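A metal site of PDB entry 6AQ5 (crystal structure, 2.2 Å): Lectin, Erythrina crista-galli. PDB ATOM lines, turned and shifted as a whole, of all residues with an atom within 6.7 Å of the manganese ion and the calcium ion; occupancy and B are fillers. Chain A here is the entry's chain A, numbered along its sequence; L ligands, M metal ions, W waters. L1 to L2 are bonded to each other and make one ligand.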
ATOM      1  N   ASP A  89      16.601  21.387  -3.399  1.00  0.00           N
ATOM      2  CA  ASP A  89      15.253  21.951  -3.465  1.00  0.00           C
ATOM      3  C   ASP A  89      14.250  20.980  -4.113  1.00  0.00           C
ATOM      4  O   ASP A  89      13.051  21.076  -3.858  1.00  0.00           O
ATOM      5  CB  ASP A  89      15.257  23.267  -4.248  1.00  0.00           C
ATOM      6  CG  ASP A  89      15.464  24.486  -3.354  1.00  0.00           C
ATOM      7  OD1 ASP A  89      16.607  24.982  -3.291  1.00  0.00           O
ATOM      8  OD2 ASP A  89      14.491  24.931  -2.723  1.00  0.00           O
ATOM      9  N   TYR A 106      17.212  26.968  -7.185  1.00  0.00           N
ATOM     10  CA  TYR A 106      16.633  26.919  -5.831  1.00  0.00           C
ATOM     11  C   TYR A 106      15.183  26.435  -5.959  1.00  0.00           C
ATOM     12  O   TYR A 106      14.926  25.505  -6.727  1.00  0.00           O
ATOM     13  CB  TYR A 106      16.817  28.281  -5.136  1.00  0.00           C
ATOM     14  CG  TYR A 106      18.224  28.833  -5.204  1.00  0.00           C
ATOM     15  CD1 TYR A 106      18.450  30.216  -5.289  1.00  0.00           C
ATOM     16  CD2 TYR A 106      19.340  28.002  -5.170  1.00  0.00           C
ATOM     17  CE1 TYR A 106      19.748  30.739  -5.363  1.00  0.00           C
ATOM     18  CE2 TYR A 106      20.641  28.521  -5.235  1.00  0.00           C
ATOM     19  CZ  TYR A 106      20.841  29.887  -5.331  1.00  0.00           C
ATOM     20  OH  TYR A 106      22.108  30.409  -5.385  1.00  0.00           O
ATOM     21  N   GLY A 107      14.222  27.052  -5.255  1.00  0.00           N
ATOM     22  CA  GLY A 107      12.855  26.572  -5.255  1.00  0.00           C
ATOM     23  C   GLY A 107      12.122  26.764  -6.564  1.00  0.00           C
ATOM     24  O   GLY A 107      10.982  26.303  -6.679  1.00  0.00           O
ATOM     25  N   TYR A 108      12.739  27.423  -7.526  1.00  0.00           N
ATOM     26  CA  TYR A 108      12.175  27.484  -8.871  1.00  0.00           C
ATOM     27  C   TYR A 108      12.606  26.298  -9.729  1.00  0.00           C
ATOM     28  O   TYR A 108      12.175  26.194 -10.884  1.00  0.00           O
ATOM     29  CB  TYR A 108      12.577  28.812  -9.546  1.00  0.00           C
ATOM     30  CG  TYR A 108      12.320  30.010  -8.652  1.00  0.00           C
ATOM     31  CD1 TYR A 108      11.035  30.397  -8.317  1.00  0.00           C
ATOM     32  CD2 TYR A 108      13.385  30.737  -8.112  1.00  0.00           C
ATOM     33  CE1 TYR A 108      10.800  31.466  -7.483  1.00  0.00           C
ATOM     34  CE2 TYR A 108      13.159  31.810  -7.279  1.00  0.00           C
ATOM     35  CZ  TYR A 108      11.860  32.177  -6.962  1.00  0.00           C
ATOM     36  OH  TYR A 108      11.632  33.255  -6.137  1.00  0.00           O
ATOM     37  N   LEU A 109      13.437  25.413  -9.185  1.00  0.00           N
ATOM     38  CA  LEU A 109      13.712  24.083  -9.722  1.00  0.00           C
ATOM     39  C   LEU A 109      14.276  24.130 -11.142  1.00  0.00           C
ATOM     40  O   LEU A 109      14.276  23.109 -11.835  1.00  0.00           O
ATOM     41  CB  LEU A 109      12.453  23.210  -9.663  1.00  0.00           C
ATOM     42  CG  LEU A 109      11.861  23.029  -8.268  1.00  0.00           C
ATOM     43  CD1 LEU A 109      10.620  22.155  -8.296  1.00  0.00           C
ATOM     44  CD2 LEU A 109      12.892  22.436  -7.298  1.00  0.00           C
ATOM     45  N   GLU A 127       6.154  18.246 -10.044  1.00  0.00           N
ATOM     46  CA  GLU A 127       7.328  18.490  -9.225  1.00  0.00           C
ATOM     47  C   GLU A 127       7.390  17.512  -8.058  1.00  0.00           C
ATOM     48  O   GLU A 127       6.372  17.033  -7.569  1.00  0.00           O
ATOM     49  CB  GLU A 127       7.348  19.921  -8.690  1.00  0.00           C
ATOM     50  CG  GLU A 127       6.202  20.233  -7.749  1.00  0.00           C
ATOM     51  CD  GLU A 127       6.366  21.548  -7.014  1.00  0.00           C
ATOM     52  OE1 GLU A 127       6.744  22.552  -7.649  1.00  0.00           O
ATOM     53  OE2 GLU A 127       6.139  21.582  -5.792  1.00  0.00           O
ATOM     54  N   ASP A 129       9.102  18.082  -4.657  1.00  0.00           N
ATOM     55  CA  ASP A 129       9.632  19.285  -4.018  1.00  0.00           C
ATOM     56  C   ASP A 129      10.058  18.938  -2.592  1.00  0.00           C
ATOM     57  O   ASP A 129       9.256  18.439  -1.806  1.00  0.00           O
ATOM     58  CB  ASP A 129       8.561  20.378  -4.038  1.00  0.00           C
ATOM     59  CG  ASP A 129       9.065  21.713  -3.544  1.00  0.00           C
ATOM     60  OD1 ASP A 129      10.194  21.803  -3.010  1.00  0.00           O
ATOM     61  OD2 ASP A 129       8.307  22.707  -3.695  1.00  0.00           O
ATOM     62  N   THR A 130      11.320  19.238  -2.258  1.00  0.00           N
ATOM     63  CA  THR A 130      11.878  18.849  -0.974  1.00  0.00           C
ATOM     64  C   THR A 130      12.072  19.991   0.013  1.00  0.00           C
ATOM     65  O   THR A 130      12.440  19.731   1.164  1.00  0.00           O
ATOM     66  CB  THR A 130      13.231  18.140  -1.191  1.00  0.00           C
ATOM     67  OG1 THR A 130      14.087  18.975  -1.973  1.00  0.00           O
ATOM     68  CG2 THR A 130      13.027  16.816  -1.919  1.00  0.00           C
ATOM     69  N   PHE A 131      11.831  21.241  -0.394  1.00  0.00           N
ATOM     70  CA  PHE A 131      11.987  22.378   0.497  1.00  0.00           C
ATOM     71  C   PHE A 131      10.741  23.253   0.465  1.00  0.00           C
ATOM     72  O   PHE A 131      10.247  23.578  -0.616  1.00  0.00           O
ATOM     73  CB  PHE A 131      13.222  23.214   0.125  1.00  0.00           C
ATOM     74  CG  PHE A 131      13.449  24.392   1.039  1.00  0.00           C
ATOM     75  CD1 PHE A 131      14.256  24.277   2.156  1.00  0.00           C
ATOM     76  CD2 PHE A 131      12.834  25.612   0.786  1.00  0.00           C
ATOM     77  CE1 PHE A 131      14.449  25.355   3.006  1.00  0.00           C
ATOM     78  CE2 PHE A 131      13.021  26.702   1.632  1.00  0.00           C
ATOM     79  CZ  PHE A 131      13.835  26.572   2.739  1.00  0.00           C
ATOM     80  N   SER A 132      10.250  23.633   1.640  1.00  0.00           N
ATOM     81  CA  SER A 132       9.012  24.413   1.743  1.00  0.00           C
ATOM     82  C   SER A 132       9.343  25.892   1.595  1.00  0.00           C
ATOM     83  O   SER A 132       9.759  26.551   2.561  1.00  0.00           O
ATOM     84  CB  SER A 132       8.299  24.124   3.050  1.00  0.00           C
ATOM     85  OG  SER A 132       7.027  24.751   3.074  1.00  0.00           O
ATOM     86  N   ASN A 133       9.169  26.417   0.394  1.00  0.00           N
ATOM     87  CA  ASN A 133       9.309  27.839   0.111  1.00  0.00           C
ATOM     88  C   ASN A 133       8.047  28.572   0.569  1.00  0.00           C
ATOM     89  O   ASN A 133       7.045  27.945   0.908  1.00  0.00           O
ATOM     90  CB  ASN A 133       9.556  28.036  -1.382  1.00  0.00           C
ATOM     91  CG  ASN A 133      10.912  27.528  -1.835  1.00  0.00           C
ATOM     92  OD1 ASN A 133      11.914  28.237  -1.727  1.00  0.00           O
ATOM     93  ND2 ASN A 133      10.946  26.314  -2.358  1.00  0.00           N
ATOM     94  N   TRP A 135       5.779  29.967  -1.006  1.00  0.00           N
ATOM     95  CA  TRP A 135       4.637  29.648  -1.862  1.00  0.00           C
ATOM     96  C   TRP A 135       4.207  28.182  -1.783  1.00  0.00           C
ATOM     97  O   TRP A 135       3.301  27.778  -2.507  1.00  0.00           O
ATOM     98  CB  TRP A 135       4.971  29.996  -3.316  1.00  0.00           C
ATOM     99  CG  TRP A 135       6.269  29.398  -3.786  1.00  0.00           C
ATOM    100  CD1 TRP A 135       6.461  28.135  -4.264  1.00  0.00           C
ATOM    101  CD2 TRP A 135       7.549  30.037  -3.818  1.00  0.00           C
ATOM    102  NE1 TRP A 135       7.777  27.944  -4.590  1.00  0.00           N
ATOM    103  CE2 TRP A 135       8.474  29.094  -4.329  1.00  0.00           C
ATOM    104  CE3 TRP A 135       8.019  31.308  -3.464  1.00  0.00           C
ATOM    105  CZ2 TRP A 135       9.828  29.388  -4.501  1.00  0.00           C
ATOM    106  CZ3 TRP A 135       9.364  31.598  -3.635  1.00  0.00           C
ATOM    107  CH2 TRP A 135      10.250  30.646  -4.139  1.00  0.00           C
ATOM    108  N   ASP A 136       4.844  27.376  -0.919  1.00  0.00           N
ATOM    109  CA  ASP A 136       4.632  25.944  -0.806  1.00  0.00           C
ATOM    110  C   ASP A 136       3.697  25.614   0.337  1.00  0.00           C
ATOM    111  O   ASP A 136       3.504  26.415   1.266  1.00  0.00           O
ATOM    112  CB  ASP A 136       5.971  25.234  -0.556  1.00  0.00           C
ATOM    113  CG  ASP A 136       6.761  25.028  -1.824  1.00  0.00           C
ATOM    114  OD1 ASP A 136       6.135  24.741  -2.862  1.00  0.00           O
ATOM    115  OD2 ASP A 136       8.002  25.145  -1.774  1.00  0.00           O
ATOM    116  N   PRO A 137       3.086  24.431   0.324  1.00  0.00           N
ATOM    117  CA  PRO A 137       2.494  23.893   1.550  1.00  0.00           C
ATOM    118  C   PRO A 137       3.570  23.641   2.587  1.00  0.00           C
ATOM    119  O   PRO A 137       4.765  23.614   2.241  1.00  0.00           O
ATOM    120  CB  PRO A 137       1.835  22.588   1.083  1.00  0.00           C
ATOM    121  CG  PRO A 137       2.602  22.200  -0.132  1.00  0.00           C
ATOM    122  CD  PRO A 137       2.968  23.487  -0.805  1.00  0.00           C
ATOM    123  N   VAL A 140       7.048  18.847   3.410  1.00  0.00           N
ATOM    124  CA  VAL A 140       7.975  18.401   2.374  1.00  0.00           C
ATOM    125  C   VAL A 140       8.478  17.011   2.760  1.00  0.00           C
ATOM    126  O   VAL A 140       8.588  16.695   3.947  1.00  0.00           O
ATOM    127  CB  VAL A 140       9.143  19.381   2.187  1.00  0.00           C
ATOM    128  CG1 VAL A 140       8.673  20.601   1.416  1.00  0.00           C
ATOM    129  CG2 VAL A 140       9.734  19.786   3.529  1.00  0.00           C
ATOM    130  N   HIS A 142       6.787  16.913  -1.232  1.00  0.00           N
ATOM    131  CA  HIS A 142       5.432  16.812  -1.762  1.00  0.00           C
ATOM    132  C   HIS A 142       5.501  16.725  -3.265  1.00  0.00           C
ATOM    133  O   HIS A 142       6.408  17.278  -3.904  1.00  0.00           O
ATOM    134  CB  HIS A 142       4.545  17.996  -1.326  1.00  0.00           C
ATOM    135  CG  HIS A 142       5.079  19.340  -1.719  1.00  0.00           C
ATOM    136  ND1 HIS A 142       5.661  20.203  -0.826  1.00  0.00           N
ATOM    137  CD2 HIS A 142       5.097  19.973  -2.923  1.00  0.00           C
ATOM    138  CE1 HIS A 142       6.022  21.317  -1.447  1.00  0.00           C
ATOM    139  NE2 HIS A 142       5.691  21.193  -2.723  1.00  0.00           N
ATOM    140  N   ILE A 143       4.552  15.981  -3.837  1.00  0.00           N
ATOM    141  CA  ILE A 143       4.292  16.040  -5.273  1.00  0.00           C
ATOM    142  C   ILE A 143       3.462  17.267  -5.563  1.00  0.00           C
ATOM    143  O   ILE A 143       2.589  17.637  -4.767  1.00  0.00           O
ATOM    144  CB  ILE A 143       3.582  14.771  -5.753  1.00  0.00           C
ATOM    145  CG1 ILE A 143       4.196  13.508  -5.115  1.00  0.00           C
ATOM    146  CG2 ILE A 143       3.621  14.673  -7.277  1.00  0.00           C
ATOM    147  CD1 ILE A 143       3.397  12.243  -5.381  1.00  0.00           C
ATOM    148  N   GLY A 144       3.711  17.912  -6.690  1.00  0.00           N
ATOM    149  CA  GLY A 144       2.908  19.045  -7.071  1.00  0.00           C
ATOM    150  C   GLY A 144       2.642  19.089  -8.548  1.00  0.00           C
ATOM    151  O   GLY A 144       3.513  18.769  -9.364  1.00  0.00           O
ATOM    152  N   ASP A 146       2.140  21.604 -11.380  1.00  0.00           N
ATOM    153  CA  ASP A 146       2.472  22.994 -11.643  1.00  0.00           C
ATOM    154  C   ASP A 146       1.950  23.387 -13.028  1.00  0.00           C
ATOM    155  O   ASP A 146       2.390  22.828 -14.035  1.00  0.00           O
ATOM    156  CB  ASP A 146       3.976  23.236 -11.572  1.00  0.00           C
ATOM    157  CG  ASP A 146       4.550  22.918 -10.211  1.00  0.00           C
ATOM    158  OD1 ASP A 146       3.776  22.690  -9.260  1.00  0.00           O
ATOM    159  OD2 ASP A 146       5.798  22.882 -10.113  1.00  0.00           O
ATOM    160  N   ILE A 150       5.316  27.994 -10.262  1.00  0.00           N
ATOM    161  CA  ILE A 150       5.913  27.126  -9.267  1.00  0.00           C
ATOM    162  C   ILE A 150       4.946  26.889  -8.114  1.00  0.00           C
ATOM    163  O   ILE A 150       5.093  25.911  -7.366  1.00  0.00           O
ATOM    164  CB  ILE A 150       7.257  27.698  -8.773  1.00  0.00           C
ATOM    165  CG1 ILE A 150       8.023  26.654  -7.965  1.00  0.00           C
ATOM    166  CG2 ILE A 150       7.027  28.947  -7.942  1.00  0.00           C
ATOM    167  CD1 ILE A 150       8.453  25.434  -8.747  1.00  0.00           C
ATOM    168  N   ARG A 151       3.948  27.754  -7.945  1.00  0.00           N
ATOM    169  CA  ARG A 151       2.904  27.592  -6.940  1.00  0.00           C
ATOM    170  C   ARG A 151       1.889  26.588  -7.485  1.00  0.00           C
ATOM    171  O   ARG A 151       1.066  26.917  -8.337  1.00  0.00           O
ATOM    172  CB  ARG A 151       2.246  28.933  -6.620  1.00  0.00           C
ATOM    173  CG  ARG A 151       1.222  28.864  -5.491  1.00  0.00           C
ATOM    174  CD  ARG A 151       0.490  30.206  -5.300  1.00  0.00           C
ATOM    175  NE  ARG A 151       1.405  31.295  -4.995  1.00  0.00           N
ATOM    176  CZ  ARG A 151       1.700  31.702  -3.774  1.00  0.00           C
ATOM    177  NH1 ARG A 151       1.155  31.114  -2.715  1.00  0.00           N
ATOM    178  NH2 ARG A 151       2.545  32.713  -3.593  1.00  0.00           N
ATOM    179  N   SER A 152       1.953  25.352  -6.982  1.00  0.00           N
ATOM    180  CA  SER A 152       1.188  24.258  -7.554  1.00  0.00           C
ATOM    181  C   SER A 152      -0.309  24.486  -7.388  1.00  0.00           C
ATOM    182  O   SER A 152      -0.770  25.019  -6.376  1.00  0.00           O
ATOM    183  CB  SER A 152       1.569  22.934  -6.878  1.00  0.00           C
ATOM    184  OG  SER A 152       2.975  22.764  -6.838  1.00  0.00           O
ATOM    185  N   THR A 155      -1.121  19.839  -4.494  1.00  0.00           N
ATOM    186  CA  THR A 155       0.043  19.195  -3.891  1.00  0.00           C
ATOM    187  C   THR A 155      -0.381  17.977  -3.107  1.00  0.00           C
ATOM    188  O   THR A 155      -1.515  17.893  -2.604  1.00  0.00           O
ATOM    189  CB  THR A 155       0.819  20.146  -2.966  1.00  0.00           C
ATOM    190  OG1 THR A 155      -0.037  20.584  -1.909  1.00  0.00           O
ATOM    191  CG2 THR A 155       1.339  21.348  -3.740  1.00  0.00           C
HETATM  192  C1  LIG L   1      18.980  33.770   2.116  1.00  0.00           C
HETATM  193  C2  LIG L   1      19.597  32.424   2.350  1.00  0.00           C
HETATM  194  C3  LIG L   1      19.066  31.435   1.333  1.00  0.00           C
HETATM  195  C4  LIG L   1      17.556  31.509   1.216  1.00  0.00           C
HETATM  196  C5  LIG L   1      17.004  32.925   1.311  1.00  0.00           C
HETATM  197  C6  LIG L   1      15.515  32.863   1.583  1.00  0.00           C
HETATM  198  O1  LIG L   1      19.528  34.686   3.022  1.00  0.00           O
HETATM  199  O2  LIG L   1      19.256  31.976   3.640  1.00  0.00           O
HETATM  200  O3  LIG L   1      19.446  30.145   1.736  1.00  0.00           O
HETATM  201  O4  LIG L   1      17.190  30.921  -0.006  1.00  0.00           O
HETATM  202  O5  LIG L   1      17.599  33.661   2.355  1.00  0.00           O
HETATM  203  O6  LIG L   1      14.869  33.964   1.001  1.00  0.00           O
HETATM  204  C1  LG2 L   2      16.461  29.727   0.138  1.00  0.00           C
HETATM  205  C2  LG2 L   2      15.883  29.297  -1.197  1.00  0.00           C
HETATM  206  C3  LG2 L   2      15.143  27.987  -1.016  1.00  0.00           C
HETATM  207  C4  LG2 L   2      16.089  26.951  -0.454  1.00  0.00           C
HETATM  208  C5  LG2 L   2      16.721  27.449   0.829  1.00  0.00           C
HETATM  209  C6  LG2 L   2      17.805  26.477   1.243  1.00  0.00           C
HETATM  210  O1  LG2 L   2      14.984  30.265  -1.679  1.00  0.00           O
HETATM  211  O2  LG2 L   2      14.629  27.550  -2.257  1.00  0.00           O
HETATM  212  O3  LG2 L   2      17.117  26.682  -1.384  1.00  0.00           O
HETATM  213  O4  LG2 L   2      17.311  28.721   0.627  1.00  0.00           O
HETATM  214  O5  LG2 L   2      18.284  26.806   2.533  1.00  0.00           O
HETATM  215 MN    MN M   1       6.145  22.975  -4.157  1.00  0.00          MN
HETATM  216 CA    CA M   2       9.895  24.305  -2.810  1.00  0.00          CA
HETATM  217  O   HOH W   1       9.457  25.421  -4.922  1.00  0.00           O
HETATM  218  O   HOH W   2       6.775  24.380  -5.929  1.00  0.00           O
HETATM  219  O   HOH W   3      12.184  23.858  -3.429  1.00  0.00           O
HETATM  220  O   HOH W   4       3.995  23.188  -4.663  1.00  0.00           O
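The manganese ion is bound by OE2 of Glu 127 (2.1 Å), OD1 of Asp 136 (2.2 Å), water W4 (2.2 Å), OD2 of Asp 129 (2.2 Å), NE2 of His 142 (2.3 Å) and water W2 (2.3 Å).
The calcium ion is bound by the side-chain amide nitrogen (ND2) of Asn 133 (2.3 Å), the side-chain carboxylate (OD2) of Asp 136 (2.3 Å), the backbone carbonyl oxygen (O) of Phe 131 (2.3 Å), water W3 (2.4 Å), the side-chain carboxylate (OD2) of Asp 129 (2.4 Å), water W1 (2.4 Å) and the side-chain carboxylate (OD1) of Asp 129 (2.5 Å).
Four residues have an atom within 4 Å of the calcium ion: Asp 129, Phe 131, Asn 133 and Asp 136. The nearest printed residue that does not touch the calcium ion is Gly 107 (4.5 Å).
Water W2 lies within hydrogen-bond range of OE1 of Glu 127 and O of Ile 150. Water W1 lies within hydrogen-bond range of O of Gly 107 and NE1 of Trp 135.
Within 4 Å of the manganese ion: Glu 127, Asp 129, Asp 136 and His 142.
OD2 of Asp 146 lies close to OE1 of Glu 127 (2.7 Å). The backbone NH (N) of Glu 127 lies within hydrogen-bond range of the backbone carbonyl oxygen (O) of Gly 144.
An oxygen (O2) of LG2 L2 lies within hydrogen-bond range of the side-chain amide oxygen of Asn 133 (2.9 Å). N of Gly 107 is in hydrogen-bond range of O2 of LG2 L2, 3.1 Å away. An oxygen (O3) of LG2 L2 sits at hydrogen-bond distance from the side-chain carboxylate of Asp 89 (2.6 Å).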
